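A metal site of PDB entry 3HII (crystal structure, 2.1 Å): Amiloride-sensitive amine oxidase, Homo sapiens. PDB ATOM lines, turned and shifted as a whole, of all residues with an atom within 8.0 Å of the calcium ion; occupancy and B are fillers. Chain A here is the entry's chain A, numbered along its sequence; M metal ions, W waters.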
ATOM      1  N   LYS A  59       6.192 -11.819  30.054  1.00  0.00           N
ATOM      2  CA  LYS A  59       7.130 -11.185  29.117  1.00  0.00           C
ATOM      3  C   LYS A  59       6.610  -9.828  28.648  1.00  0.00           C
ATOM      4  O   LYS A  59       7.378  -8.881  28.530  1.00  0.00           O
ATOM      5  CB  LYS A  59       7.375 -12.118  27.922  1.00  0.00           C
ATOM      6  CG  LYS A  59       8.369 -11.607  26.854  1.00  0.00           C
ATOM      7  CD  LYS A  59       8.704 -12.760  25.867  1.00  0.00           C
ATOM      8  CE  LYS A  59       9.597 -12.313  24.707  1.00  0.00           C
ATOM      9  NZ  LYS A  59       9.854 -13.403  23.704  1.00  0.00           N
ATOM     10  N   ARG A 325      18.841  -6.632  21.329  1.00  0.00           N
ATOM     11  CA  ARG A 325      18.423  -7.928  21.839  1.00  0.00           C
ATOM     12  C   ARG A 325      18.618  -9.014  20.790  1.00  0.00           C
ATOM     13  O   ARG A 325      18.406  -8.808  19.587  1.00  0.00           O
ATOM     14  CB  ARG A 325      16.972  -7.918  22.332  1.00  0.00           C
ATOM     15  CG  ARG A 325      16.589  -9.186  23.086  1.00  0.00           C
ATOM     16  CD  ARG A 325      15.228  -9.092  23.780  1.00  0.00           C
ATOM     17  NE  ARG A 325      15.242  -8.157  24.916  1.00  0.00           N
ATOM     18  CZ  ARG A 325      14.573  -6.996  24.976  1.00  0.00           C
ATOM     19  NH1 ARG A 325      13.789  -6.599  23.980  1.00  0.00           N
ATOM     20  NH2 ARG A 325      14.673  -6.223  26.044  1.00  0.00           N
ATOM     21  N   ILE A 326      19.038 -10.165  21.275  1.00  0.00           N
ATOM     22  CA  ILE A 326      19.221 -11.367  20.472  1.00  0.00           C
ATOM     23  C   ILE A 326      18.304 -12.498  20.963  1.00  0.00           C
ATOM     24  O   ILE A 326      17.672 -13.169  20.148  1.00  0.00           O
ATOM     25  CB  ILE A 326      20.676 -11.812  20.567  1.00  0.00           C
ATOM     26  CG1 ILE A 326      21.555 -10.802  19.834  1.00  0.00           C
ATOM     27  CG2 ILE A 326      20.859 -13.197  19.972  1.00  0.00           C
ATOM     28  CD1 ILE A 326      23.014 -10.942  20.174  1.00  0.00           C
ATOM     29  N   ALA A 327      18.227 -12.669  22.286  1.00  0.00           N
ATOM     30  CA  ALA A 327      17.409 -13.713  22.910  1.00  0.00           C
ATOM     31  C   ALA A 327      16.785 -13.240  24.237  1.00  0.00           C
ATOM     32  O   ALA A 327      17.488 -12.755  25.112  1.00  0.00           O
ATOM     33  CB  ALA A 327      18.246 -14.960  23.163  1.00  0.00           C
ATOM     34  N   TYR A 328      15.473 -13.418  24.390  1.00  0.00           N
ATOM     35  CA  TYR A 328      14.831 -13.113  25.666  1.00  0.00           C
ATOM     36  C   TYR A 328      15.163 -14.154  26.736  1.00  0.00           C
ATOM     37  O   TYR A 328      15.274 -13.802  27.916  1.00  0.00           O
ATOM     38  CB  TYR A 328      13.314 -13.010  25.503  1.00  0.00           C
ATOM     39  CG  TYR A 328      12.612 -12.594  26.776  1.00  0.00           C
ATOM     40  CD1 TYR A 328      12.630 -11.264  27.178  1.00  0.00           C
ATOM     41  CD2 TYR A 328      11.944 -13.511  27.578  1.00  0.00           C
ATOM     42  CE1 TYR A 328      12.000 -10.861  28.346  1.00  0.00           C
ATOM     43  CE2 TYR A 328      11.304 -13.117  28.748  1.00  0.00           C
ATOM     44  CZ  TYR A 328      11.338 -11.779  29.124  1.00  0.00           C
ATOM     45  OH  TYR A 328      10.736 -11.349  30.270  1.00  0.00           O
ATOM     46  N   GLU A 329      15.330 -15.415  26.326  1.00  0.00           N
ATOM     47  CA  GLU A 329      15.605 -16.519  27.246  1.00  0.00           C
ATOM     48  C   GLU A 329      16.296 -17.659  26.521  1.00  0.00           C
ATOM     49  O   GLU A 329      15.943 -18.006  25.386  1.00  0.00           O
ATOM     50  CB  GLU A 329      14.294 -17.030  27.862  1.00  0.00           C
ATOM     51  CG  GLU A 329      14.446 -18.178  28.906  1.00  0.00           C
ATOM     52  CD  GLU A 329      13.147 -18.939  29.143  1.00  0.00           C
ATOM     53  OE1 GLU A 329      12.104 -18.481  28.632  1.00  0.00           O
ATOM     54  OE2 GLU A 329      13.160 -19.998  29.813  1.00  0.00           O
ATOM     55  N   ARG A 497      15.166 -24.462  25.774  1.00  0.00           N
ATOM     56  CA  ARG A 497      14.251 -23.434  25.276  1.00  0.00           C
ATOM     57  C   ARG A 497      15.090 -22.263  24.841  1.00  0.00           C
ATOM     58  O   ARG A 497      15.916 -21.752  25.606  1.00  0.00           O
ATOM     59  CB  ARG A 497      13.292 -22.980  26.371  1.00  0.00           C
ATOM     60  CG  ARG A 497      12.290 -21.893  25.926  1.00  0.00           C
ATOM     61  CD  ARG A 497      11.422 -21.456  27.096  1.00  0.00           C
ATOM     62  NE  ARG A 497      10.679 -20.217  26.850  1.00  0.00           N
ATOM     63  CZ  ARG A 497       9.479 -20.124  26.270  1.00  0.00           C
ATOM     64  NH1 ARG A 497       8.843 -21.211  25.840  1.00  0.00           N
ATOM     65  NH2 ARG A 497       8.904 -18.936  26.110  1.00  0.00           N
ATOM     66  N   VAL A 498      14.880 -21.824  23.612  1.00  0.00           N
ATOM     67  CA  VAL A 498      15.698 -20.779  23.026  1.00  0.00           C
ATOM     68  C   VAL A 498      14.790 -19.707  22.448  1.00  0.00           C
ATOM     69  O   VAL A 498      14.480 -19.689  21.261  1.00  0.00           O
ATOM     70  CB  VAL A 498      16.682 -21.348  21.981  1.00  0.00           C
ATOM     71  CG1 VAL A 498      17.721 -20.303  21.609  1.00  0.00           C
ATOM     72  CG2 VAL A 498      17.361 -22.623  22.504  1.00  0.00           C
ATOM     73  N   ASP A 499      14.337 -18.809  23.325  1.00  0.00           N
ATOM     74  CA  ASP A 499      13.414 -17.744  22.936  1.00  0.00           C
ATOM     75  C   ASP A 499      14.243 -16.619  22.330  1.00  0.00           C
ATOM     76  O   ASP A 499      14.611 -15.662  22.997  1.00  0.00           O
ATOM     77  CB  ASP A 499      12.613 -17.253  24.141  1.00  0.00           C
ATOM     78  CG  ASP A 499      11.593 -16.167  23.776  1.00  0.00           C
ATOM     79  OD1 ASP A 499      11.421 -15.875  22.568  1.00  0.00           O
ATOM     80  OD2 ASP A 499      10.950 -15.631  24.699  1.00  0.00           O
ATOM     81  N   LEU A 500      14.554 -16.774  21.043  1.00  0.00           N
ATOM     82  CA  LEU A 500      15.274 -15.746  20.308  1.00  0.00           C
ATOM     83  C   LEU A 500      14.303 -14.589  20.007  1.00  0.00           C
ATOM     84  O   LEU A 500      13.165 -14.817  19.598  1.00  0.00           O
ATOM     85  CB  LEU A 500      15.867 -16.306  19.013  1.00  0.00           C
ATOM     86  CG  LEU A 500      16.982 -17.353  19.203  1.00  0.00           C
ATOM     87  CD1 LEU A 500      17.121 -18.275  17.998  1.00  0.00           C
ATOM     88  CD2 LEU A 500      18.326 -16.691  19.546  1.00  0.00           C
ATOM     89  N   ASP A 501      14.763 -13.360  20.258  1.00  0.00           N
ATOM     90  CA  ASP A 501      14.090 -12.141  19.841  1.00  0.00           C
ATOM     91  C   ASP A 501      15.111 -11.356  19.009  1.00  0.00           C
ATOM     92  O   ASP A 501      15.750 -10.431  19.500  1.00  0.00           O
ATOM     93  CB  ASP A 501      13.652 -11.282  21.037  1.00  0.00           C
ATOM     94  CG  ASP A 501      12.449 -11.822  21.766  1.00  0.00           C
ATOM     95  OD1 ASP A 501      11.885 -12.879  21.420  1.00  0.00           O
ATOM     96  OD2 ASP A 501      12.047 -11.152  22.744  1.00  0.00           O
ATOM     97  N   VAL A 502      15.242 -11.714  17.746  1.00  0.00           N
ATOM     98  CA  VAL A 502      16.328 -11.173  16.934  1.00  0.00           C
ATOM     99  C   VAL A 502      16.035  -9.715  16.582  1.00  0.00           C
ATOM    100  O   VAL A 502      15.075  -9.418  15.877  1.00  0.00           O
ATOM    101  CB  VAL A 502      16.599 -12.047  15.699  1.00  0.00           C
ATOM    102  CG1 VAL A 502      17.834 -11.558  14.963  1.00  0.00           C
ATOM    103  CG2 VAL A 502      16.752 -13.539  16.136  1.00  0.00           C
ATOM    104  N   GLY A 504      14.522  -7.721  18.272  1.00  0.00           N
ATOM    105  CA  GLY A 504      13.099  -7.486  18.543  1.00  0.00           C
ATOM    106  C   GLY A 504      12.301  -8.771  18.659  1.00  0.00           C
ATOM    107  O   GLY A 504      12.787  -9.860  18.335  1.00  0.00           O
ATOM    108  N   THR A 505      11.066  -8.622  19.126  1.00  0.00           N
ATOM    109  CA  THR A 505      10.156  -9.739  19.341  1.00  0.00           C
ATOM    110  C   THR A 505       9.762 -10.435  18.043  1.00  0.00           C
ATOM    111  O   THR A 505       9.769 -11.651  17.961  1.00  0.00           O
ATOM    112  CB  THR A 505       8.889  -9.221  20.054  1.00  0.00           C
ATOM    113  OG1 THR A 505       9.268  -8.254  21.044  1.00  0.00           O
ATOM    114  CG2 THR A 505       8.139 -10.350  20.702  1.00  0.00           C
ATOM    115  N   LYS A 506       9.411  -9.646  17.018  1.00  0.00           N
ATOM    116  CA  LYS A 506       8.846 -10.205  15.776  1.00  0.00           C
ATOM    117  C   LYS A 506       9.908 -10.735  14.799  1.00  0.00           C
ATOM    118  O   LYS A 506      10.663  -9.960  14.204  1.00  0.00           O
ATOM    119  CB  LYS A 506       7.963  -9.188  15.059  1.00  0.00           C
ATOM    120  CG  LYS A 506       6.738  -8.734  15.873  1.00  0.00           C
ATOM    121  CD  LYS A 506       5.639  -9.802  15.920  1.00  0.00           C
ATOM    122  CE  LYS A 506       4.330  -9.249  16.463  1.00  0.00           C
ATOM    123  NZ  LYS A 506       3.829  -8.084  15.655  1.00  0.00           N
ATOM    124  N   ASN A 507       9.914 -12.047  14.643  1.00  0.00           N
ATOM    125  CA  ASN A 507      10.840 -12.743  13.769  1.00  0.00           C
ATOM    126  C   ASN A 507      10.158 -13.706  12.798  1.00  0.00           C
ATOM    127  O   ASN A 507       8.949 -13.996  12.896  1.00  0.00           O
ATOM    128  CB  ASN A 507      11.833 -13.556  14.609  1.00  0.00           C
ATOM    129  CG  ASN A 507      12.717 -12.695  15.494  1.00  0.00           C
ATOM    130  OD1 ASN A 507      13.133 -13.125  16.586  1.00  0.00           O
ATOM    131  ND2 ASN A 507      13.063 -11.505  15.013  1.00  0.00           N
ATOM    132  N   PHE A 559      16.976 -17.469  12.192  1.00  0.00           N
ATOM    133  CA  PHE A 559      15.897 -16.686  12.786  1.00  0.00           C
ATOM    134  C   PHE A 559      16.134 -15.239  12.425  1.00  0.00           C
ATOM    135  O   PHE A 559      17.165 -14.671  12.782  1.00  0.00           O
ATOM    136  CB  PHE A 559      15.806 -16.935  14.278  1.00  0.00           C
ATOM    137  CG  PHE A 559      15.443 -18.360  14.590  1.00  0.00           C
ATOM    138  CD1 PHE A 559      16.386 -19.362  14.504  1.00  0.00           C
ATOM    139  CD2 PHE A 559      14.138 -18.707  14.914  1.00  0.00           C
ATOM    140  CE1 PHE A 559      16.043 -20.685  14.751  1.00  0.00           C
ATOM    141  CE2 PHE A 559      13.789 -20.005  15.150  1.00  0.00           C
ATOM    142  CZ  PHE A 559      14.745 -21.010  15.066  1.00  0.00           C
ATOM    143  N   THR A 605       8.018 -22.701  17.942  1.00  0.00           N
ATOM    144  CA  THR A 605       6.627 -22.397  18.320  1.00  0.00           C
ATOM    145  C   THR A 605       6.351 -20.911  18.417  1.00  0.00           C
ATOM    146  O   THR A 605       7.262 -20.097  18.534  1.00  0.00           O
ATOM    147  CB  THR A 605       6.193 -23.087  19.647  1.00  0.00           C
ATOM    148  OG1 THR A 605       7.012 -22.650  20.749  1.00  0.00           O
ATOM    149  CG2 THR A 605       6.260 -24.606  19.507  1.00  0.00           C
ATOM    150  N   LYS A 606       5.082 -20.546  18.333  1.00  0.00           N
ATOM    151  CA  LYS A 606       4.664 -19.188  18.642  1.00  0.00           C
ATOM    152  C   LYS A 606       4.645 -19.008  20.160  1.00  0.00           C
ATOM    153  O   LYS A 606       4.069 -19.824  20.875  1.00  0.00           O
ATOM    154  CB  LYS A 606       3.282 -18.926  18.071  1.00  0.00           C
ATOM    155  CG  LYS A 606       2.673 -17.588  18.504  1.00  0.00           C
ATOM    156  CD  LYS A 606       1.445 -17.280  17.675  1.00  0.00           C
ATOM    157  CE  LYS A 606       0.651 -16.118  18.285  1.00  0.00           C
ATOM    158  NZ  LYS A 606      -0.143 -15.492  17.206  1.00  0.00           N
ATOM    159  N   TYR A 607       5.285 -17.946  20.639  1.00  0.00           N
ATOM    160  CA  TYR A 607       5.356 -17.642  22.073  1.00  0.00           C
ATOM    161  C   TYR A 607       3.971 -17.624  22.746  1.00  0.00           C
ATOM    162  O   TYR A 607       2.999 -17.156  22.170  1.00  0.00           O
ATOM    163  CB  TYR A 607       6.041 -16.300  22.323  1.00  0.00           C
ATOM    164  CG  TYR A 607       6.202 -15.989  23.797  1.00  0.00           C
ATOM    165  CD1 TYR A 607       5.195 -15.344  24.506  1.00  0.00           C
ATOM    166  CD2 TYR A 607       7.371 -16.354  24.491  1.00  0.00           C
ATOM    167  CE1 TYR A 607       5.332 -15.081  25.864  1.00  0.00           C
ATOM    168  CE2 TYR A 607       7.512 -16.075  25.850  1.00  0.00           C
ATOM    169  CZ  TYR A 607       6.492 -15.444  26.532  1.00  0.00           C
ATOM    170  OH  TYR A 607       6.640 -15.191  27.864  1.00  0.00           O
ATOM    171  N   GLU A 643       6.284 -13.154  13.909  1.00  0.00           N
ATOM    172  CA  GLU A 643       5.717 -13.485  15.223  1.00  0.00           C
ATOM    173  C   GLU A 643       6.847 -13.641  16.235  1.00  0.00           C
ATOM    174  O   GLU A 643       8.017 -13.754  15.866  1.00  0.00           O
ATOM    175  CB  GLU A 643       4.918 -14.807  15.166  1.00  0.00           C
ATOM    176  CG  GLU A 643       3.594 -14.741  14.406  1.00  0.00           C
ATOM    177  CD  GLU A 643       2.456 -14.138  15.212  1.00  0.00           C
ATOM    178  OE1 GLU A 643       2.283 -14.510  16.394  1.00  0.00           O
ATOM    179  OE2 GLU A 643       1.725 -13.304  14.664  1.00  0.00           O
ATOM    180  N   ASP A 644       6.483 -13.614  17.507  1.00  0.00           N
ATOM    181  CA  ASP A 644       7.385 -13.936  18.599  1.00  0.00           C
ATOM    182  C   ASP A 644       7.584 -15.460  18.596  1.00  0.00           C
ATOM    183  O   ASP A 644       6.667 -16.204  18.984  1.00  0.00           O
ATOM    184  CB  ASP A 644       6.802 -13.455  19.922  1.00  0.00           C
ATOM    185  CG  ASP A 644       7.772 -13.603  21.088  1.00  0.00           C
ATOM    186  OD1 ASP A 644       8.835 -14.231  20.911  1.00  0.00           O
ATOM    187  OD2 ASP A 644       7.456 -13.100  22.181  1.00  0.00           O
ATOM    188  N   LEU A 645       8.761 -15.905  18.169  1.00  0.00           N
ATOM    189  CA  LEU A 645       9.067 -17.333  18.008  1.00  0.00           C
ATOM    190  C   LEU A 645       9.926 -17.852  19.157  1.00  0.00           C
ATOM    191  O   LEU A 645      10.728 -17.114  19.732  1.00  0.00           O
ATOM    192  CB  LEU A 645       9.817 -17.589  16.681  1.00  0.00           C
ATOM    193  CG  LEU A 645       9.207 -17.013  15.393  1.00  0.00           C
ATOM    194  CD1 LEU A 645      10.088 -17.340  14.161  1.00  0.00           C
ATOM    195  CD2 LEU A 645       7.784 -17.545  15.189  1.00  0.00           C
ATOM    196  N   VAL A 646       9.751 -19.130  19.475  1.00  0.00           N
ATOM    197  CA  VAL A 646      10.638 -19.837  20.378  1.00  0.00           C
ATOM    198  C   VAL A 646      11.200 -21.050  19.643  1.00  0.00           C
ATOM    199  O   VAL A 646      10.447 -21.843  19.115  1.00  0.00           O
ATOM    200  CB  VAL A 646       9.864 -20.298  21.627  1.00  0.00           C
ATOM    201  CG1 VAL A 646      10.781 -21.049  22.577  1.00  0.00           C
ATOM    202  CG2 VAL A 646       9.189 -19.079  22.308  1.00  0.00           C
ATOM    203  N   ALA A 647      12.527 -21.162  19.574  1.00  0.00           N
ATOM    204  CA  ALA A 647      13.178 -22.368  19.079  1.00  0.00           C
ATOM    205  C   ALA A 647      13.352 -23.319  20.257  1.00  0.00           C
ATOM    206  O   ALA A 647      13.655 -22.898  21.368  1.00  0.00           O
ATOM    207  CB  ALA A 647      14.545 -22.046  18.452  1.00  0.00           C
HETATM  208 CA    CA M   1      11.038 -14.910  20.506  1.00  0.00          CA
HETATM  209  O   HOH W   1      10.876 -13.861  18.234  1.00  0.00           O
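NZ of Lys 59 touches the calcium ion (3.7 Å). Within 4 Å of the calcium ion: Lys 59, Asp 499, Leu 500, Asp 501, Asp 644 and Leu 645. The nearest printed residue that does not touch the calcium ion is Thr 505 (4.3 Å).
Water W1 lies within hydrogen-bond range of the backbone carbonyl oxygen (O) of Thr 505 (2.5 Å), the side-chain amide oxygen (OD1) of Asn 507 (2.9 Å) and the backbone NH (N) of Leu 645 (2.9 Å).
The side-chain amide oxygen (OD1) of Asn 507 lies close to the backbone carbonyl oxygen (O) of Leu 500, 3.5 Å away. NZ of Lys 59 lies within salt-bridge range of OD2 of Asp 499 (2.7 Å). O of Asp 644 is in hydrogen-bond range of N of Tyr 607 (2.8 Å). The side-chain carboxylate (OD2) of Asp 644 is in salt-bridge range of the side-chain amino group (NZ) of Lys 59. The side-chain carboxylate (OD2) of Asp 501 lies within salt-bridge range of the side-chain amino group (NZ) of Lys 59 (3.3 Å). N of Asp 501 is in hydrogen-bond range of O of Ile 326. The backbone carbonyl oxygen (O) of Asp 499 is in hydrogen-bond range of the backbone NH (N) of Tyr 328, at 2.8 Å. The backbone carbonyl oxygen (O) of Glu 329 lies within hydrogen-bond range of the backbone NH (N) of Asp 499 (2.7 Å).
The calcium ion is bound by the side-chain carboxylate (OD1) of Asp 499 (2.3 Å), the backbone carbonyl oxygen (O) of Leu 500 (2.3 Å), the side-chain carboxylate (OD1) of Asp 644 (2.3 Å), the backbone carbonyl oxygen (O) of Leu 645 (2.4 Å), the side-chain carboxylate (OD1) of Asp 501 (2.4 Å) and water W1 (2.5 Å).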
